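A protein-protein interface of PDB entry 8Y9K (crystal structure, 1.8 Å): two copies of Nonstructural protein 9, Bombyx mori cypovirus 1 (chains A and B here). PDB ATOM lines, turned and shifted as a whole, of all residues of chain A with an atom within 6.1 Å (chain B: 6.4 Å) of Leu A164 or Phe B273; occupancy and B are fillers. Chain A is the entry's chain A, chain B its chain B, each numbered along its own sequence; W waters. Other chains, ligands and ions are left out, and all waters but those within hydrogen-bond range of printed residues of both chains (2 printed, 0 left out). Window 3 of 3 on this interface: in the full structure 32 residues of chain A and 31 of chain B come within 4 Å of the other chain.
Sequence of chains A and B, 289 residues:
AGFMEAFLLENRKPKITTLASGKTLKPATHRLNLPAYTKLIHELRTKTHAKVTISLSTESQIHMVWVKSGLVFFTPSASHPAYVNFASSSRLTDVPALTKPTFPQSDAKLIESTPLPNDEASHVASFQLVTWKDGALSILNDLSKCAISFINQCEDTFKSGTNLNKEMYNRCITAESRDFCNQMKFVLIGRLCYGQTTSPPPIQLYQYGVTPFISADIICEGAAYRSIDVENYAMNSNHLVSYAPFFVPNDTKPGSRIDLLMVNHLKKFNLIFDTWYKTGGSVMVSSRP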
ATOM      1  N   ASP A 156      21.609  23.675  -9.872  1.00  0.00           N
ATOM      2  CA  ASP A 156      21.491  22.564 -10.810  1.00  0.00           C
ATOM      3  C   ASP A 156      22.504  21.466 -10.478  1.00  0.00           C
ATOM      4  O   ASP A 156      22.190  20.271 -10.539  1.00  0.00           O
ATOM      5  CB  ASP A 156      21.695  23.044 -12.251  1.00  0.00           C
ATOM      6  CG  ASP A 156      20.672  24.077 -12.702  1.00  0.00           C
ATOM      7  OD1 ASP A 156      19.808  24.488 -11.904  1.00  0.00           O
ATOM      8  OD2 ASP A 156      20.751  24.492 -13.876  1.00  0.00           O
ATOM      9  N   THR A 157      23.732  21.858 -10.119  1.00  0.00           N
ATOM     10  CA  THR A 157      24.824  20.899  -9.972  1.00  0.00           C
ATOM     11  C   THR A 157      24.798  20.193  -8.622  1.00  0.00           C
ATOM     12  O   THR A 157      25.072  18.991  -8.548  1.00  0.00           O
ATOM     13  CB  THR A 157      26.165  21.609 -10.184  1.00  0.00           C
ATOM     14  OG1 THR A 157      26.171  22.213 -11.488  1.00  0.00           O
ATOM     15  CG2 THR A 157      27.324  20.642 -10.078  1.00  0.00           C
ATOM     16  N   PHE A 158      24.491  20.913  -7.544  1.00  0.00           N
ATOM     17  CA  PHE A 158      24.648  20.359  -6.210  1.00  0.00           C
ATOM     18  C   PHE A 158      23.341  20.043  -5.506  1.00  0.00           C
ATOM     19  O   PHE A 158      23.367  19.318  -4.505  1.00  0.00           O
ATOM     20  CB  PHE A 158      25.475  21.321  -5.348  1.00  0.00           C
ATOM     21  CG  PHE A 158      26.842  21.564  -5.897  1.00  0.00           C
ATOM     22  CD1 PHE A 158      27.833  20.612  -5.721  1.00  0.00           C
ATOM     23  CD2 PHE A 158      27.129  22.704  -6.615  1.00  0.00           C
ATOM     24  CE1 PHE A 158      29.093  20.813  -6.225  1.00  0.00           C
ATOM     25  CE2 PHE A 158      28.392  22.915  -7.133  1.00  0.00           C
ATOM     26  CZ  PHE A 158      29.378  21.964  -6.939  1.00  0.00           C
ATOM     27  N   THR A 162      21.504  15.465  -9.593  1.00  0.00           N
ATOM     28  CA  THR A 162      22.112  15.126 -10.867  1.00  0.00           C
ATOM     29  C   THR A 162      23.354  14.281 -10.623  1.00  0.00           C
ATOM     30  O   THR A 162      24.142  14.556  -9.711  1.00  0.00           O
ATOM     31  CB  THR A 162      22.500  16.401 -11.622  1.00  0.00           C
ATOM     32  OG1 THR A 162      21.329  17.018 -12.166  1.00  0.00           O
ATOM     33  CG2 THR A 162      23.481  16.092 -12.749  1.00  0.00           C
ATOM     34  N   ASN A 163      23.532  13.249 -11.442  1.00  0.00           N
ATOM     35  CA  ASN A 163      24.750  12.466 -11.357  1.00  0.00           C
ATOM     36  C   ASN A 163      25.923  13.393 -11.623  1.00  0.00           C
ATOM     37  O   ASN A 163      25.885  14.229 -12.530  1.00  0.00           O
ATOM     38  CB  ASN A 163      24.733  11.326 -12.373  1.00  0.00           C
ATOM     39  N   LEU A 164      26.976  13.240 -10.841  1.00  0.00           N
ATOM     40  CA  LEU A 164      28.162  14.053 -11.024  1.00  0.00           C
ATOM     41  C   LEU A 164      29.395  13.167 -11.029  1.00  0.00           C
ATOM     42  O   LEU A 164      29.395  12.054 -10.498  1.00  0.00           O
ATOM     43  CB  LEU A 164      28.338  15.149  -9.959  1.00  0.00           C
ATOM     44  CG  LEU A 164      27.209  16.046  -9.461  1.00  0.00           C
ATOM     45  CD1 LEU A 164      27.793  16.970  -8.383  1.00  0.00           C
ATOM     46  CD2 LEU A 164      26.624  16.846 -10.587  1.00  0.00           C
ATOM     47  N   ASN A 165      30.389  13.626 -11.780  1.00  0.00           N
ATOM     48  CA  ASN A 165      31.721  13.037 -11.761  1.00  0.00           C
ATOM     49  C   ASN A 165      32.370  13.309 -10.401  1.00  0.00           C
ATOM     50  O   ASN A 165      32.354  14.444  -9.911  1.00  0.00           O
ATOM     51  CB  ASN A 165      32.531  13.637 -12.901  1.00  0.00           C
ATOM     52  CG  ASN A 165      33.935  13.105 -12.953  1.00  0.00           C
ATOM     53  OD1 ASN A 165      34.668  13.112 -11.972  1.00  0.00           O
ATOM     54  ND2 ASN A 165      34.337  12.668 -14.140  1.00  0.00           N
ATOM     55  N   LYS A 166      32.880  12.249  -9.760  1.00  0.00           N
ATOM     56  CA  LYS A 166      33.441  12.407  -8.416  1.00  0.00           C
ATOM     57  C   LYS A 166      34.629  13.355  -8.408  1.00  0.00           C
ATOM     58  O   LYS A 166      34.780  14.180  -7.498  1.00  0.00           O
ATOM     59  CB  LYS A 166      33.879  11.061  -7.839  1.00  0.00           C
ATOM     60  CG  LYS A 166      34.027  11.036  -6.309  1.00  0.00           C
ATOM     61  CD  LYS A 166      34.306   9.618  -5.829  1.00  0.00           C
ATOM     62  CE  LYS A 166      35.798   9.220  -5.979  1.00  0.00           C
ATOM     63  NZ  LYS A 166      36.326   8.550  -4.765  1.00  0.00           N
ATOM     64  N   GLU A 167      35.509  13.227  -9.392  1.00  0.00           N
ATOM     65  CA  GLU A 167      36.683  14.096  -9.445  1.00  0.00           C
ATOM     66  C   GLU A 167      36.275  15.550  -9.631  1.00  0.00           C
ATOM     67  O   GLU A 167      36.814  16.442  -8.968  1.00  0.00           O
ATOM     68  CB  GLU A 167      37.608  13.641 -10.573  1.00  0.00           C
ATOM     69  N   TYR A 169      33.420  16.916  -8.831  1.00  0.00           N
ATOM     70  CA  TYR A 169      32.798  17.365  -7.587  1.00  0.00           C
ATOM     71  C   TYR A 169      33.846  17.841  -6.590  1.00  0.00           C
ATOM     72  O   TYR A 169      33.742  18.940  -6.031  1.00  0.00           O
ATOM     73  CB  TYR A 169      31.974  16.229  -6.991  1.00  0.00           C
ATOM     74  CG  TYR A 169      31.475  16.500  -5.604  1.00  0.00           C
ATOM     75  CD1 TYR A 169      30.476  17.439  -5.369  1.00  0.00           C
ATOM     76  CD2 TYR A 169      31.995  15.820  -4.516  1.00  0.00           C
ATOM     77  CE1 TYR A 169      30.010  17.680  -4.092  1.00  0.00           C
ATOM     78  CE2 TYR A 169      31.540  16.061  -3.242  1.00  0.00           C
ATOM     79  CZ  TYR A 169      30.544  16.991  -3.034  1.00  0.00           C
ATOM     80  OH  TYR A 169      30.090  17.231  -1.766  1.00  0.00           O
ATOM     81  N   LEU B 266      28.873   8.485   5.582  1.00  0.00           N
ATOM     82  CA  LEU B 266      27.731   9.381   5.765  1.00  0.00           C
ATOM     83  C   LEU B 266      27.421  10.068   4.439  1.00  0.00           C
ATOM     84  O   LEU B 266      28.324  10.620   3.803  1.00  0.00           O
ATOM     85  CB  LEU B 266      27.982  10.433   6.847  1.00  0.00           C
ATOM     86  CG  LEU B 266      28.176   9.928   8.278  1.00  0.00           C
ATOM     87  CD1 LEU B 266      28.439  11.072   9.233  1.00  0.00           C
ATOM     88  CD2 LEU B 266      26.955   9.110   8.732  1.00  0.00           C
ATOM     89  N   LYS B 267      26.150  10.020   4.017  1.00  0.00           N
ATOM     90  CA  LYS B 267      25.758  10.564   2.720  1.00  0.00           C
ATOM     91  C   LYS B 267      25.774  12.085   2.782  1.00  0.00           C
ATOM     92  O   LYS B 267      25.283  12.673   3.750  1.00  0.00           O
ATOM     93  CB  LYS B 267      24.363  10.073   2.357  1.00  0.00           C
ATOM     94  CG  LYS B 267      23.909  10.330   0.958  1.00  0.00           C
ATOM     95  CD  LYS B 267      24.795   9.586  -0.022  1.00  0.00           C
ATOM     96  CE  LYS B 267      24.347   8.124  -0.149  1.00  0.00           C
ATOM     97  NZ  LYS B 267      25.370   7.219  -0.748  1.00  0.00           N
ATOM     98  N   LYS B 268      26.409  12.727   1.804  1.00  0.00           N
ATOM     99  CA  LYS B 268      26.450  14.185   1.787  1.00  0.00           C
ATOM    100  C   LYS B 268      25.099  14.754   1.357  1.00  0.00           C
ATOM    101  O   LYS B 268      24.205  14.041   0.895  1.00  0.00           O
ATOM    102  CB  LYS B 268      27.590  14.685   0.895  1.00  0.00           C
ATOM    103  CG  LYS B 268      28.939  14.255   1.442  1.00  0.00           C
ATOM    104  CD  LYS B 268      30.116  14.659   0.563  1.00  0.00           C
ATOM    105  CE  LYS B 268      30.610  15.972   1.123  1.00  0.00           C
ATOM    106  NZ  LYS B 268      31.758  16.634   0.495  1.00  0.00           N
ATOM    107  N   PHE B 269      24.955  16.070   1.504  1.00  0.00           N
ATOM    108  CA  PHE B 269      23.668  16.690   1.237  1.00  0.00           C
ATOM    109  C   PHE B 269      23.274  16.611  -0.227  1.00  0.00           C
ATOM    110  O   PHE B 269      22.079  16.695  -0.539  1.00  0.00           O
ATOM    111  CB  PHE B 269      23.717  18.130   1.709  1.00  0.00           C
ATOM    112  CG  PHE B 269      23.781  18.270   3.188  1.00  0.00           C
ATOM    113  CD1 PHE B 269      22.790  17.720   3.982  1.00  0.00           C
ATOM    114  CD2 PHE B 269      24.841  18.918   3.788  1.00  0.00           C
ATOM    115  CE1 PHE B 269      22.825  17.859   5.353  1.00  0.00           C
ATOM    116  CE2 PHE B 269      24.904  19.045   5.165  1.00  0.00           C
ATOM    117  CZ  PHE B 269      23.900  18.512   5.951  1.00  0.00           C
ATOM    118  N   ASN B 270      24.236  16.469  -1.132  1.00  0.00           N
ATOM    119  CA  ASN B 270      23.862  16.295  -2.530  1.00  0.00           C
ATOM    120  C   ASN B 270      23.255  14.916  -2.781  1.00  0.00           C
ATOM    121  O   ASN B 270      22.747  14.673  -3.881  1.00  0.00           O
ATOM    122  CB  ASN B 270      25.083  16.515  -3.409  1.00  0.00           C
ATOM    123  CG  ASN B 270      26.269  15.670  -2.997  1.00  0.00           C
ATOM    124  OD1 ASN B 270      26.252  14.446  -3.128  1.00  0.00           O
ATOM    125  ND2 ASN B 270      27.283  16.317  -2.433  1.00  0.00           N
ATOM    126  N   LEU B 271      23.384  13.986  -1.817  1.00  0.00           N
ATOM    127  CA  LEU B 271      22.805  12.642  -1.820  1.00  0.00           C
ATOM    128  C   LEU B 271      23.450  11.708  -2.836  1.00  0.00           C
ATOM    129  O   LEU B 271      22.923  10.625  -3.096  1.00  0.00           O
ATOM    130  CB  LEU B 271      21.287  12.644  -2.009  1.00  0.00           C
ATOM    131  CG  LEU B 271      20.496  13.544  -1.060  1.00  0.00           C
ATOM    132  CD1 LEU B 271      18.994  13.421  -1.293  1.00  0.00           C
ATOM    133  CD2 LEU B 271      20.877  13.165   0.394  1.00  0.00           C
ATOM    134  N   ILE B 272      24.564  12.107  -3.438  1.00  0.00           N
ATOM    135  CA  ILE B 272      25.301  11.274  -4.383  1.00  0.00           C
ATOM    136  C   ILE B 272      26.561  10.721  -3.741  1.00  0.00           C
ATOM    137  O   ILE B 272      26.844   9.529  -3.831  1.00  0.00           O
ATOM    138  CB  ILE B 272      25.629  12.025  -5.697  1.00  0.00           C
ATOM    139  CG1 ILE B 272      24.347  12.587  -6.302  1.00  0.00           C
ATOM    140  CG2 ILE B 272      26.372  11.105  -6.658  1.00  0.00           C
ATOM    141  CD1 ILE B 272      23.386  11.504  -6.788  1.00  0.00           C
ATOM    142  N   PHE B 273      27.341  11.577  -3.107  1.00  0.00           N
ATOM    143  CA  PHE B 273      28.639  11.206  -2.576  1.00  0.00           C
ATOM    144  C   PHE B 273      28.585  11.084  -1.063  1.00  0.00           C
ATOM    145  O   PHE B 273      27.607  11.489  -0.422  1.00  0.00           O
ATOM    146  CB  PHE B 273      29.644  12.277  -2.968  1.00  0.00           C
ATOM    147  CG  PHE B 273      29.784  12.440  -4.448  1.00  0.00           C
ATOM    148  CD1 PHE B 273      30.318  11.427  -5.217  1.00  0.00           C
ATOM    149  CD2 PHE B 273      29.333  13.604  -5.069  1.00  0.00           C
ATOM    150  CE1 PHE B 273      30.446  11.577  -6.578  1.00  0.00           C
ATOM    151  CE2 PHE B 273      29.446  13.764  -6.444  1.00  0.00           C
ATOM    152  CZ  PHE B 273      30.004  12.748  -7.202  1.00  0.00           C
ATOM    153  N   ASP B 274      29.614  10.445  -0.509  1.00  0.00           N
ATOM    154  CA  ASP B 274      29.667  10.154   0.912  1.00  0.00           C
ATOM    155  C   ASP B 274      30.982  10.662   1.489  1.00  0.00           C
ATOM    156  O   ASP B 274      32.010  10.751   0.803  1.00  0.00           O
ATOM    157  CB  ASP B 274      29.527   8.655   1.208  1.00  0.00           C
ATOM    158  CG  ASP B 274      28.200   8.096   0.812  1.00  0.00           C
ATOM    159  OD1 ASP B 274      27.276   8.243   1.609  1.00  0.00           O
ATOM    160  OD2 ASP B 274      28.087   7.479  -0.276  1.00  0.00           O
ATOM    161  N   THR B 275      30.951  10.901   2.792  1.00  0.00           N
ATOM    162  CA  THR B 275      32.147  11.113   3.591  1.00  0.00           C
ATOM    163  C   THR B 275      32.500   9.776   4.236  1.00  0.00           C
ATOM    164  O   THR B 275      31.655   9.150   4.888  1.00  0.00           O
ATOM    165  CB  THR B 275      31.879  12.197   4.634  1.00  0.00           C
ATOM    166  OG1 THR B 275      31.623  13.432   3.950  1.00  0.00           O
ATOM    167  CG2 THR B 275      33.079  12.395   5.509  1.00  0.00           C
HETATM  168  O   HOH W   1      22.417  16.731  -6.031  1.00  0.00           O
HETATM  169  O   HOH W   2      24.330  19.666  -1.937  1.00  0.00           O
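OH of Tyr A169 lies within hydrogen-bond range of NZ of Lys B268, 2.9 Å away.
OH of Tyr A169 is in hydrogen-bond range of ND2 of Asn B270, 3.0 Å away.
The side-chain amide oxygen (OD1) of Asn B270 is in hydrogen-bond range of the backbone NH (N) of Ile B272 (2.9 Å).
OD1 of Asn A165 lies within hydrogen-bond range of N of Glu A167 (2.7 Å).
The side-chain amide oxygen (OD1) of Asn B270 is in hydrogen-bond range of the backbone NH (N) of Phe B273 (3.1 Å).
N of Lys B268 is in hydrogen-bond range of O of Phe B273.
Among the printed residues, pairs that only touch across the chains: Leu A164 with Phe B273 (3.4 Å), Phe A158 with Asn B270 (3.5 Å), Tyr A169 with Phe B273 (3.5 Å), Lys A166 with Phe B273 (3.6 Å), Thr A162 with Ile B272 (3.9 Å) and Asn A165 with Phe B273 (3.97 Å).
Of the printed residues of chain B, Phe A158 touches Asn B270.
Of chain B, only Phe B273 (3.4 Å) comes within 4 Å of Leu A164.
Printed residues of chain B within 4 Å of Lys A166: Phe B273.
Of the printed residues of chain B, Tyr A169 touches Lys B268, Asn B270 and Phe B273.
Of the printed residues of chain A, Lys B268 touches Tyr A169 (2.9 Å).
Of the printed residues of chain A, Ile B272 touches Thr A162.
Hydrophobic or aromatic side chains of chain B that line the printed part of chain A: Ile B272 and Phe B273.
Printed residues of chain A that touch a printed residue of chain B: Phe A158, Thr A162, Leu A164, Asn A165, Lys A166 and Tyr A169.
Hydrophobic or aromatic side chains of chain A that line the printed part of chain B: Leu A164 and Tyr A169.
Among the printed residues, 8 pairs touch across the chains.
No position is printed for both chains.
Of the 8 pairs that touch across the chains among the printed residues, none has its exchanged pair printed and touching as well.
Water W2 bridges O of Phe A158 (2.8 Å) and N of Asn B270 (3.3 Å).
Water W1 bridges O of Asn B270 (3.0 Å) and O of Phe A158 (3.2 Å).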
